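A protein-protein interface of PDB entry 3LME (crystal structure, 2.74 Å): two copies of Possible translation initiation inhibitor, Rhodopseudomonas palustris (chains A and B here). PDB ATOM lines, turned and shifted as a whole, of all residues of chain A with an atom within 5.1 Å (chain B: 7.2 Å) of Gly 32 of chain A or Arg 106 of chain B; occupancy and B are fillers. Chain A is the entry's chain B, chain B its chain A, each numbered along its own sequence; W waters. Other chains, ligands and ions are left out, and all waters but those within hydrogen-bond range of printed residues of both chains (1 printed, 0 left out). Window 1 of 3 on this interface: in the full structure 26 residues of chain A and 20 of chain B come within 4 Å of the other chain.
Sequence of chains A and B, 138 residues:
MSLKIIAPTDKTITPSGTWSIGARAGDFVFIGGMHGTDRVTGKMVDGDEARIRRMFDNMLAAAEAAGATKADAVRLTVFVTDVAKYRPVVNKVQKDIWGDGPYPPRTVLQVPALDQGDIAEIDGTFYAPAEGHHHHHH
1 position is printed for both chains.
Printed residues of chain B within 4 Å of Gly 22 of chain A: Pro 105 (3.4 Å). Printed residues of chain B within 4 Å of Gly 32 of chain A: Pro 105 and Arg 106. Val 90 of chain B touches none of the printed residues of chain A. Of the printed residues of chain A, Gln 94 of chain B touches Thr 18 (3.4 Å). Of the printed residues of chain A, Pro 104 of chain B touches Trp 19 (3.5 Å) and Ser 20 (3.5 Å). Of chain A, only Thr 18 (3.2 Å), Trp 19 (3.4 Å), Gly 32 (3.9 Å) and Gly 33 (3.2 Å) come within 4 Å of Arg 106 of chain B. Ile 122 of chain B touches none of the printed residues of chain A. The nearest printed residue of chain A that does not touch Asn 91 of chain B is Trp 19 of chain A (5.5 Å).
Water W1 lies within hydrogen-bond range of O of Pro 104 of chain B (2.7 Å), O of Thr 18 of chain A (2.7 Å) and NE2 of Gln 94 of chain B (2.9 Å).
Among the printed residues, merely in contact across the chains: Asp 123 of chain A with Thr 107 of chain B (3.1 Å), Trp 19 of chain A with Arg 106 of chain B (3.4 Å), Trp 19 of chain A with Tyr 103 of chain B (3.4 Å), Gly 22 of chain A with Pro 105 of chain B (3.4 Å), Ser 20 of chain A with Pro 104 of chain B (3.5 Å), Trp 19 of chain A with Pro 104 of chain B (3.5 Å), Thr 18 of chain A with Tyr 103 of chain B (3.5 Å), Phe 30 of chain A with Val 74 of chain B (3.5 Å), Ser 20 of chain A with Pro 105 of chain B (3.6 Å), Gly 32 of chain A with Pro 105 of chain B (3.8 Å), Phe 30 of chain A with Arg 75 of chain B (3.8 Å), Asp 123 of chain A with Arg 75 of chain B (3.9 Å), Gly 32 of chain A with Arg 106 of chain B (3.9 Å), Gly 33 of chain A with Thr 107 of chain B (3.9 Å) and Phe 30 of chain A with Pro 105 of chain B (3.998 Å).
The backbone carbonyl oxygen (O) of Arg 87 of chain B lies close to the side-chain amide nitrogen (ND2) of Asn 91 of chain B (3.5 Å). NH2 of Arg 106 of chain B is in hydrogen-bond range of OE1 of Gln 94 of chain B, at 2.8 Å. The side-chain amide oxygen of Asn 91 of chain B sits at hydrogen-bond distance from the guanidinium group of Arg 106 of chain B (2.9 Å). N of Val 78 of chain B is in hydrogen-bond range of O of Thr 107 of chain B (2.8 Å). O of Ile 21 of chain A lies within hydrogen-bond range of N of Gly 32 of chain A, at 3.0 Å. The backbone carbonyl oxygen (O) of Leu 76 of chain B is in hydrogen-bond range of the backbone NH (N) of Thr 107 of chain B (2.9 Å).
Of the 18 printed residues of chain B, 9 touch a printed residue of chain A. Hydrophobic or aromatic side chains of chain A within 4 Å of the printed part of chain B: Trp 19 and Phe 30.
The side-chain amide oxygen (OD1) of Asn 91 of chain B lies within hydrogen-bond range of the side-chain hydroxyl (OG1) of Thr 18 of chain A (3.4 Å). OG of Ser 20 of chain A is in hydrogen-bond range of O of Tyr 103 of chain B (2.6 Å). The guanidinium group (NH2) of Arg 75 of chain B is in hydrogen-bond range of the backbone carbonyl oxygen (O) of Ile 31 of chain A, at 2.8 Å. NH2 of Arg 106 of chain B sits at hydrogen-bond distance from OG1 of Thr 18 of chain A (3.2 Å). The backbone carbonyl oxygen (O) of Arg 106 of chain B sits at hydrogen-bond distance from the backbone NH (N) of Gly 33 of chain A, at 3.2 Å. OE1 of Gln 94 of chain B is in hydrogen-bond range of OG1 of Thr 18 of chain A (3.4 Å).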
ATOM      1  N   THR A  18     -23.347   2.645 -11.910  1.00  0.00           N
ATOM      2  CA  THR A  18     -24.051   3.692 -12.636  1.00  0.00           C
ATOM      3  C   THR A  18     -23.187   4.932 -12.733  1.00  0.00           C
ATOM      4  O   THR A  18     -23.524   5.994 -12.215  1.00  0.00           O
ATOM      5  CB  THR A  18     -25.461   3.978 -12.043  1.00  0.00           C
ATOM      6  OG1 THR A  18     -25.353   4.443 -10.688  1.00  0.00           O
ATOM      7  CG2 THR A  18     -26.310   2.721 -12.051  1.00  0.00           C
ATOM      8  N   TRP A  19     -22.042   4.785 -13.392  1.00  0.00           N
ATOM      9  CA  TRP A  19     -21.084   5.895 -13.549  1.00  0.00           C
ATOM     10  C   TRP A  19     -20.066   5.606 -14.656  1.00  0.00           C
ATOM     11  O   TRP A  19     -20.002   4.506 -15.187  1.00  0.00           O
ATOM     12  CB  TRP A  19     -20.364   6.148 -12.229  1.00  0.00           C
ATOM     13  CG  TRP A  19     -19.885   4.883 -11.566  1.00  0.00           C
ATOM     14  CD1 TRP A  19     -20.586   4.098 -10.691  1.00  0.00           C
ATOM     15  CD2 TRP A  19     -18.614   4.238 -11.754  1.00  0.00           C
ATOM     16  NE1 TRP A  19     -19.823   3.013 -10.305  1.00  0.00           N
ATOM     17  CE2 TRP A  19     -18.610   3.074 -10.941  1.00  0.00           C
ATOM     18  CE3 TRP A  19     -17.472   4.542 -12.503  1.00  0.00           C
ATOM     19  CZ2 TRP A  19     -17.488   2.218 -10.850  1.00  0.00           C
ATOM     20  CZ3 TRP A  19     -16.365   3.687 -12.418  1.00  0.00           C
ATOM     21  CH2 TRP A  19     -16.382   2.542 -11.597  1.00  0.00           C
ATOM     22  N   SER A  20     -19.283   6.617 -14.987  1.00  0.00           N
ATOM     23  CA  SER A  20     -18.269   6.582 -16.010  1.00  0.00           C
ATOM     24  C   SER A  20     -16.947   6.949 -15.404  1.00  0.00           C
ATOM     25  O   SER A  20     -16.927   7.647 -14.398  1.00  0.00           O
ATOM     26  CB  SER A  20     -18.585   7.674 -17.008  1.00  0.00           C
ATOM     27  OG  SER A  20     -19.527   7.201 -17.930  1.00  0.00           O
ATOM     28  N   ILE A  21     -15.840   6.555 -16.038  1.00  0.00           N
ATOM     29  CA  ILE A  21     -14.530   6.949 -15.544  1.00  0.00           C
ATOM     30  C   ILE A  21     -14.397   8.454 -15.625  1.00  0.00           C
ATOM     31  O   ILE A  21     -13.812   9.082 -14.743  1.00  0.00           O
ATOM     32  CB  ILE A  21     -13.361   6.263 -16.264  1.00  0.00           C
ATOM     33  CG1 ILE A  21     -13.207   6.780 -17.684  1.00  0.00           C
ATOM     34  CG2 ILE A  21     -13.538   4.758 -16.286  1.00  0.00           C
ATOM     35  CD1 ILE A  21     -11.932   6.231 -18.386  1.00  0.00           C
ATOM     36  N   GLY A  22     -14.962   9.053 -16.657  1.00  0.00           N
ATOM     37  CA  GLY A  22     -14.931  10.494 -16.727  1.00  0.00           C
ATOM     38  C   GLY A  22     -15.435  11.035 -18.028  1.00  0.00           C
ATOM     39  O   GLY A  22     -15.848  10.277 -18.898  1.00  0.00           O
ATOM     40  N   PHE A  30     -13.157  15.963 -16.923  1.00  0.00           N
ATOM     41  CA  PHE A  30     -13.571  15.697 -15.544  1.00  0.00           C
ATOM     42  C   PHE A  30     -13.491  14.223 -15.250  1.00  0.00           C
ATOM     43  O   PHE A  30     -14.136  13.448 -15.927  1.00  0.00           O
ATOM     44  CB  PHE A  30     -15.013  16.134 -15.310  1.00  0.00           C
ATOM     45  CG  PHE A  30     -15.263  17.577 -15.546  1.00  0.00           C
ATOM     46  CD1 PHE A  30     -15.372  18.455 -14.474  1.00  0.00           C
ATOM     47  CD2 PHE A  30     -15.442  18.063 -16.827  1.00  0.00           C
ATOM     48  CE1 PHE A  30     -15.647  19.825 -14.680  1.00  0.00           C
ATOM     49  CE2 PHE A  30     -15.705  19.436 -17.051  1.00  0.00           C
ATOM     50  CZ  PHE A  30     -15.815  20.315 -15.974  1.00  0.00           C
ATOM     51  N   ILE A  31     -12.714  13.835 -14.247  1.00  0.00           N
ATOM     52  CA  ILE A  31     -12.589  12.423 -13.885  1.00  0.00           C
ATOM     53  C   ILE A  31     -13.406  12.181 -12.633  1.00  0.00           C
ATOM     54  O   ILE A  31     -13.372  12.982 -11.716  1.00  0.00           O
ATOM     55  CB  ILE A  31     -11.117  12.014 -13.657  1.00  0.00           C
ATOM     56  CG1 ILE A  31     -10.221  12.501 -14.798  1.00  0.00           C
ATOM     57  CG2 ILE A  31     -10.980  10.488 -13.504  1.00  0.00           C
ATOM     58  CD1 ILE A  31     -10.732  12.150 -16.166  1.00  0.00           C
ATOM     59  N   GLY A  32     -14.178  11.105 -12.612  1.00  0.00           N
ATOM     60  CA  GLY A  32     -14.953  10.745 -11.425  1.00  0.00           C
ATOM     61  C   GLY A  32     -14.081  10.182 -10.318  1.00  0.00           C
ATOM     62  O   GLY A  32     -12.859  10.070 -10.460  1.00  0.00           O
ATOM     63  N   GLY A  33     -14.708   9.819  -9.209  1.00  0.00           N
ATOM     64  CA  GLY A  33     -13.982   9.419  -8.014  1.00  0.00           C
ATOM     65  C   GLY A  33     -13.051   8.289  -8.324  1.00  0.00           C
ATOM     66  O   GLY A  33     -13.446   7.318  -8.965  1.00  0.00           O
ATOM     67  N   MET A  34     -11.802   8.405  -7.889  1.00  0.00           N
ATOM     68  CA  MET A  34     -10.850   7.316  -8.113  1.00  0.00           C
ATOM     69  C   MET A  34     -10.358   6.758  -6.792  1.00  0.00           C
ATOM     70  O   MET A  34     -10.163   7.519  -5.874  1.00  0.00           O
ATOM     71  CB  MET A  34      -9.707   7.771  -9.022  1.00  0.00           C
ATOM     72  CG  MET A  34     -10.120   7.917 -10.487  1.00  0.00           C
ATOM     73  SD  MET A  34     -10.367   6.371 -11.373  1.00  0.00           S
ATOM     74  CE  MET A  34     -11.724   6.876 -12.388  1.00  0.00           C
ATOM     75  N   ILE A 122     -10.069  10.371  -4.842  1.00  0.00           N
ATOM     76  CA  ILE A 122      -9.689  11.664  -5.457  1.00  0.00           C
ATOM     77  C   ILE A 122     -10.567  12.094  -6.651  1.00  0.00           C
ATOM     78  O   ILE A 122     -11.044  11.278  -7.430  1.00  0.00           O
ATOM     79  CB  ILE A 122      -8.162  11.690  -5.839  1.00  0.00           C
ATOM     80  CG1 ILE A 122      -7.724  13.067  -6.316  1.00  0.00           C
ATOM     81  CG2 ILE A 122      -7.861  10.705  -6.941  1.00  0.00           C
ATOM     82  CD1 ILE A 122      -6.219  13.330  -6.253  1.00  0.00           C
ATOM     83  N   ASP A 123     -10.748  13.396  -6.783  1.00  0.00           N
ATOM     84  CA  ASP A 123     -11.552  13.999  -7.845  1.00  0.00           C
ATOM     85  C   ASP A 123     -10.675  14.920  -8.677  1.00  0.00           C
ATOM     86  O   ASP A 123     -10.335  15.991  -8.216  1.00  0.00           O
ATOM     87  CB  ASP A 123     -12.623  14.887  -7.211  1.00  0.00           C
ATOM     88  CG  ASP A 123     -13.879  14.144  -6.860  1.00  0.00           C
ATOM     89  OD1 ASP A 123     -13.970  12.928  -7.116  1.00  0.00           O
ATOM     90  OD2 ASP A 123     -14.797  14.803  -6.315  1.00  0.00           O
ATOM     91  N   PHE B  56     -32.484  14.465  -7.049  1.00  0.00           N
ATOM     92  CA  PHE B  56     -32.113  14.466  -8.465  1.00  0.00           C
ATOM     93  C   PHE B  56     -33.020  15.342  -9.348  1.00  0.00           C
ATOM     94  O   PHE B  56     -32.515  16.136 -10.162  1.00  0.00           O
ATOM     95  CB  PHE B  56     -32.046  13.059  -8.995  1.00  0.00           C
ATOM     96  CG  PHE B  56     -30.767  12.372  -8.696  1.00  0.00           C
ATOM     97  CD1 PHE B  56     -29.657  12.596  -9.470  1.00  0.00           C
ATOM     98  CD2 PHE B  56     -30.673  11.489  -7.633  1.00  0.00           C
ATOM     99  CE1 PHE B  56     -28.469  11.938  -9.203  1.00  0.00           C
ATOM    100  CE2 PHE B  56     -29.462  10.820  -7.335  1.00  0.00           C
ATOM    101  CZ  PHE B  56     -28.373  11.045  -8.112  1.00  0.00           C
ATOM    102  N   VAL B  74     -21.365  16.550 -16.427  1.00  0.00           N
ATOM    103  CA  VAL B  74     -19.941  16.170 -16.435  1.00  0.00           C
ATOM    104  C   VAL B  74     -19.428  15.777 -15.065  1.00  0.00           C
ATOM    105  O   VAL B  74     -18.399  15.131 -14.983  1.00  0.00           O
ATOM    106  CB  VAL B  74     -19.006  17.219 -17.048  1.00  0.00           C
ATOM    107  CG1 VAL B  74     -19.368  17.468 -18.507  1.00  0.00           C
ATOM    108  CG2 VAL B  74     -19.076  18.499 -16.283  1.00  0.00           C
ATOM    109  N   ARG B  75     -20.123  16.154 -13.994  1.00  0.00           N
ATOM    110  CA  ARG B  75     -19.742  15.653 -12.673  1.00  0.00           C
ATOM    111  C   ARG B  75     -20.872  15.701 -11.679  1.00  0.00           C
ATOM    112  O   ARG B  75     -21.564  16.713 -11.579  1.00  0.00           O
ATOM    113  CB  ARG B  75     -18.545  16.419 -12.078  1.00  0.00           C
ATOM    114  CG  ARG B  75     -18.012  15.797 -10.798  1.00  0.00           C
ATOM    115  CD  ARG B  75     -17.074  16.762 -10.042  1.00  0.00           C
ATOM    116  NE  ARG B  75     -15.837  16.987 -10.778  1.00  0.00           N
ATOM    117  CZ  ARG B  75     -14.915  16.053 -10.994  1.00  0.00           C
ATOM    118  NH1 ARG B  75     -13.830  16.341 -11.707  1.00  0.00           N
ATOM    119  NH2 ARG B  75     -15.084  14.832 -10.514  1.00  0.00           N
ATOM    120  N   LEU B  76     -21.019  14.619 -10.923  1.00  0.00           N
ATOM    121  CA  LEU B  76     -21.970  14.565  -9.837  1.00  0.00           C
ATOM    122  C   LEU B  76     -21.219  14.243  -8.557  1.00  0.00           C
ATOM    123  O   LEU B  76     -20.495  13.251  -8.505  1.00  0.00           O
ATOM    124  CB  LEU B  76     -23.013  13.485 -10.115  1.00  0.00           C
ATOM    125  CG  LEU B  76     -23.905  13.647 -11.353  1.00  0.00           C
ATOM    126  CD1 LEU B  76     -24.880  12.510 -11.421  1.00  0.00           C
ATOM    127  CD2 LEU B  76     -24.662  14.951 -11.290  1.00  0.00           C
ATOM    128  N   THR B  77     -21.355  15.078  -7.528  1.00  0.00           N
ATOM    129  CA  THR B  77     -20.767  14.743  -6.235  1.00  0.00           C
ATOM    130  C   THR B  77     -21.902  14.531  -5.244  1.00  0.00           C
ATOM    131  O   THR B  77     -22.583  15.464  -4.845  1.00  0.00           O
ATOM    132  CB  THR B  77     -19.731  15.813  -5.761  1.00  0.00           C
ATOM    133  OG1 THR B  77     -18.920  16.234  -6.878  1.00  0.00           O
ATOM    134  CG2 THR B  77     -18.815  15.247  -4.667  1.00  0.00           C
ATOM    135  N   VAL B  78     -22.152  13.278  -4.901  1.00  0.00           N
ATOM    136  CA  VAL B  78     -23.212  12.969  -3.960  1.00  0.00           C
ATOM    137  C   VAL B  78     -22.622  12.813  -2.567  1.00  0.00           C
ATOM    138  O   VAL B  78     -21.737  11.975  -2.337  1.00  0.00           O
ATOM    139  CB  VAL B  78     -23.968  11.702  -4.350  1.00  0.00           C
ATOM    140  CG1 VAL B  78     -25.333  11.652  -3.661  1.00  0.00           C
ATOM    141  CG2 VAL B  78     -24.156  11.659  -5.829  1.00  0.00           C
ATOM    142  N   ARG B  87     -25.941   4.302  -0.960  1.00  0.00           N
ATOM    143  CA  ARG B  87     -25.300   4.123  -2.234  1.00  0.00           C
ATOM    144  C   ARG B  87     -26.202   3.277  -3.144  1.00  0.00           C
ATOM    145  O   ARG B  87     -26.419   3.645  -4.289  1.00  0.00           O
ATOM    146  CB  ARG B  87     -23.908   3.524  -2.083  1.00  0.00           C
ATOM    147  CG  ARG B  87     -22.986   3.930  -3.193  1.00  0.00           C
ATOM    148  CD  ARG B  87     -22.033   2.846  -3.555  1.00  0.00           C
ATOM    149  NE  ARG B  87     -22.722   1.594  -3.942  1.00  0.00           N
ATOM    150  CZ  ARG B  87     -22.676   0.441  -3.249  1.00  0.00           C
ATOM    151  NH1 ARG B  87     -23.321  -0.639  -3.700  1.00  0.00           N
ATOM    152  NH2 ARG B  87     -21.976   0.363  -2.113  1.00  0.00           N
ATOM    153  N   VAL B  90     -29.099   5.533  -4.419  1.00  0.00           N
ATOM    154  CA  VAL B  90     -28.569   6.397  -5.479  1.00  0.00           C
ATOM    155  C   VAL B  90     -28.382   5.606  -6.789  1.00  0.00           C
ATOM    156  O   VAL B  90     -28.728   6.063  -7.882  1.00  0.00           O
ATOM    157  CB  VAL B  90     -27.234   7.061  -5.025  1.00  0.00           C
ATOM    158  CG1 VAL B  90     -26.597   7.848  -6.142  1.00  0.00           C
ATOM    159  CG2 VAL B  90     -27.456   7.952  -3.836  1.00  0.00           C
ATOM    160  N   ASN B  91     -27.847   4.402  -6.678  1.00  0.00           N
ATOM    161  CA  ASN B  91     -27.757   3.537  -7.834  1.00  0.00           C
ATOM    162  C   ASN B  91     -29.131   3.329  -8.473  1.00  0.00           C
ATOM    163  O   ASN B  91     -29.328   3.643  -9.659  1.00  0.00           O
ATOM    164  CB  ASN B  91     -27.082   2.215  -7.475  1.00  0.00           C
ATOM    165  CG  ASN B  91     -25.613   2.390  -7.144  1.00  0.00           C
ATOM    166  OD1 ASN B  91     -24.983   3.415  -7.442  1.00  0.00           O
ATOM    167  ND2 ASN B  91     -25.053   1.383  -6.516  1.00  0.00           N
ATOM    168  N   LYS B  92     -30.086   2.859  -7.674  1.00  0.00           N
ATOM    169  CA  LYS B  92     -31.418   2.571  -8.156  1.00  0.00           C
ATOM    170  C   LYS B  92     -32.054   3.827  -8.807  1.00  0.00           C
ATOM    171  O   LYS B  92     -32.630   3.766  -9.905  1.00  0.00           O
ATOM    172  CB  LYS B  92     -32.234   2.028  -6.985  1.00  0.00           C
ATOM    173  CG  LYS B  92     -33.707   2.100  -7.112  1.00  0.00           C
ATOM    174  CD  LYS B  92     -34.322   0.764  -7.531  1.00  0.00           C
ATOM    175  CE  LYS B  92     -35.559   1.004  -8.454  1.00  0.00           C
ATOM    176  NZ  LYS B  92     -36.229   2.372  -8.323  1.00  0.00           N
ATOM    177  N   GLN B  94     -30.562   6.411 -10.119  1.00  0.00           N
ATOM    178  CA  GLN B  94     -29.865   6.715 -11.350  1.00  0.00           C
ATOM    179  C   GLN B  94     -30.241   5.729 -12.469  1.00  0.00           C
ATOM    180  O   GLN B  94     -30.362   6.137 -13.611  1.00  0.00           O
ATOM    181  CB  GLN B  94     -28.360   6.805 -11.136  1.00  0.00           C
ATOM    182  CG  GLN B  94     -27.888   8.115 -10.566  1.00  0.00           C
ATOM    183  CD  GLN B  94     -26.389   8.285 -10.691  1.00  0.00           C
ATOM    184  OE1 GLN B  94     -25.611   7.717  -9.921  1.00  0.00           O
ATOM    185  NE2 GLN B  94     -25.969   9.071 -11.667  1.00  0.00           N
ATOM    186  N   TYR B 103     -23.640   6.906 -18.193  1.00  0.00           N
ATOM    187  CA  TYR B 103     -23.776   7.588 -16.923  1.00  0.00           C
ATOM    188  C   TYR B 103     -22.699   8.664 -16.692  1.00  0.00           C
ATOM    189  O   TYR B 103     -21.574   8.505 -17.140  1.00  0.00           O
ATOM    190  CB  TYR B 103     -23.670   6.540 -15.850  1.00  0.00           C
ATOM    191  CG  TYR B 103     -24.654   5.413 -15.967  1.00  0.00           C
ATOM    192  CD1 TYR B 103     -25.991   5.593 -15.602  1.00  0.00           C
ATOM    193  CD2 TYR B 103     -24.246   4.136 -16.398  1.00  0.00           C
ATOM    194  CE1 TYR B 103     -26.909   4.542 -15.674  1.00  0.00           C
ATOM    195  CE2 TYR B 103     -25.168   3.068 -16.472  1.00  0.00           C
ATOM    196  CZ  TYR B 103     -26.498   3.290 -16.099  1.00  0.00           C
ATOM    197  OH  TYR B 103     -27.426   2.274 -16.163  1.00  0.00           O
ATOM    198  N   PRO B 104     -23.012   9.741 -15.950  1.00  0.00           N
ATOM    199  CA  PRO B 104     -21.989  10.769 -15.714  1.00  0.00           C
ATOM    200  C   PRO B 104     -20.907  10.318 -14.731  1.00  0.00           C
ATOM    201  O   PRO B 104     -21.146   9.404 -13.938  1.00  0.00           O
ATOM    202  CB  PRO B 104     -22.765  11.922 -15.103  1.00  0.00           C
ATOM    203  CG  PRO B 104     -24.183  11.458 -15.016  1.00  0.00           C
ATOM    204  CD  PRO B 104     -24.219   9.982 -15.160  1.00  0.00           C
ATOM    205  N   PRO B 105     -19.713  10.941 -14.787  1.00  0.00           N
ATOM    206  CA  PRO B 105     -18.695  10.711 -13.782  1.00  0.00           C
ATOM    207  C   PRO B 105     -19.238  11.135 -12.418  1.00  0.00           C
ATOM    208  O   PRO B 105     -19.952  12.126 -12.315  1.00  0.00           O
ATOM    209  CB  PRO B 105     -17.569  11.656 -14.198  1.00  0.00           C
ATOM    210  CG  PRO B 105     -17.835  11.964 -15.610  1.00  0.00           C
ATOM    211  CD  PRO B 105     -19.305  11.990 -15.736  1.00  0.00           C
ATOM    212  N   ARG B 106     -18.875  10.406 -11.369  1.00  0.00           N
ATOM    213  CA  ARG B 106     -19.601  10.505 -10.130  1.00  0.00           C
ATOM    214  C   ARG B 106     -18.695  10.213  -8.959  1.00  0.00           C
ATOM    215  O   ARG B 106     -17.845   9.356  -9.043  1.00  0.00           O
ATOM    216  CB  ARG B 106     -20.744   9.480 -10.158  1.00  0.00           C
ATOM    217  CG  ARG B 106     -21.407   9.230  -8.841  1.00  0.00           C
ATOM    218  CD  ARG B 106     -22.434   8.135  -8.934  1.00  0.00           C
ATOM    219  NE  ARG B 106     -21.948   6.838  -8.501  1.00  0.00           N
ATOM    220  CZ  ARG B 106     -22.756   5.835  -8.194  1.00  0.00           C
ATOM    221  NH1 ARG B 106     -22.265   4.661  -7.815  1.00  0.00           N
ATOM    222  NH2 ARG B 106     -24.073   6.010  -8.270  1.00  0.00           N
ATOM    223  N   THR B 107     -18.904  10.901  -7.846  1.00  0.00           N
ATOM    224  CA  THR B 107     -18.227  10.553  -6.614  1.00  0.00           C
ATOM    225  C   THR B 107     -19.217  10.562  -5.439  1.00  0.00           C
ATOM    226  O   THR B 107     -19.933  11.531  -5.271  1.00  0.00           O
ATOM    227  CB  THR B 107     -16.962  11.437  -6.408  1.00  0.00           C
ATOM    228  OG1 THR B 107     -16.512  11.321  -5.065  1.00  0.00           O
ATOM    229  CG2 THR B 107     -17.250  12.890  -6.699  1.00  0.00           C
ATOM    230  N   VAL B 108     -19.275   9.467  -4.670  1.00  0.00           N
ATOM    231  CA  VAL B 108     -20.197   9.319  -3.521  1.00  0.00           C
ATOM    232  C   VAL B 108     -19.435   9.235  -2.184  1.00  0.00           C
ATOM    233  O   VAL B 108     -18.735   8.263  -1.927  1.00  0.00           O
ATOM    234  CB  VAL B 108     -21.127   8.032  -3.653  1.00  0.00           C
ATOM    235  CG1 VAL B 108     -22.041   7.882  -2.459  1.00  0.00           C
ATOM    236  CG2 VAL B 108     -21.986   8.046  -4.928  1.00  0.00           C
ATOM    237  N   ILE B 122     -26.513  16.878  -3.318  1.00  0.00           N
ATOM    238  CA  ILE B 122     -25.790  16.601  -4.555  1.00  0.00           C
ATOM    239  C   ILE B 122     -25.299  17.859  -5.223  1.00  0.00           C
ATOM    240  O   ILE B 122     -25.962  18.860  -5.156  1.00  0.00           O
ATOM    241  CB  ILE B 122     -26.613  15.698  -5.549  1.00  0.00           C
ATOM    242  CG1 ILE B 122     -25.781  15.314  -6.783  1.00  0.00           C
ATOM    243  CG2 ILE B 122     -27.898  16.384  -6.027  1.00  0.00           C
ATOM    244  CD1 ILE B 122     -26.303  14.110  -7.533  1.00  0.00           C
HETATM  245  O   HOH W   1     -23.151   8.667 -12.304  1.00  0.00           O
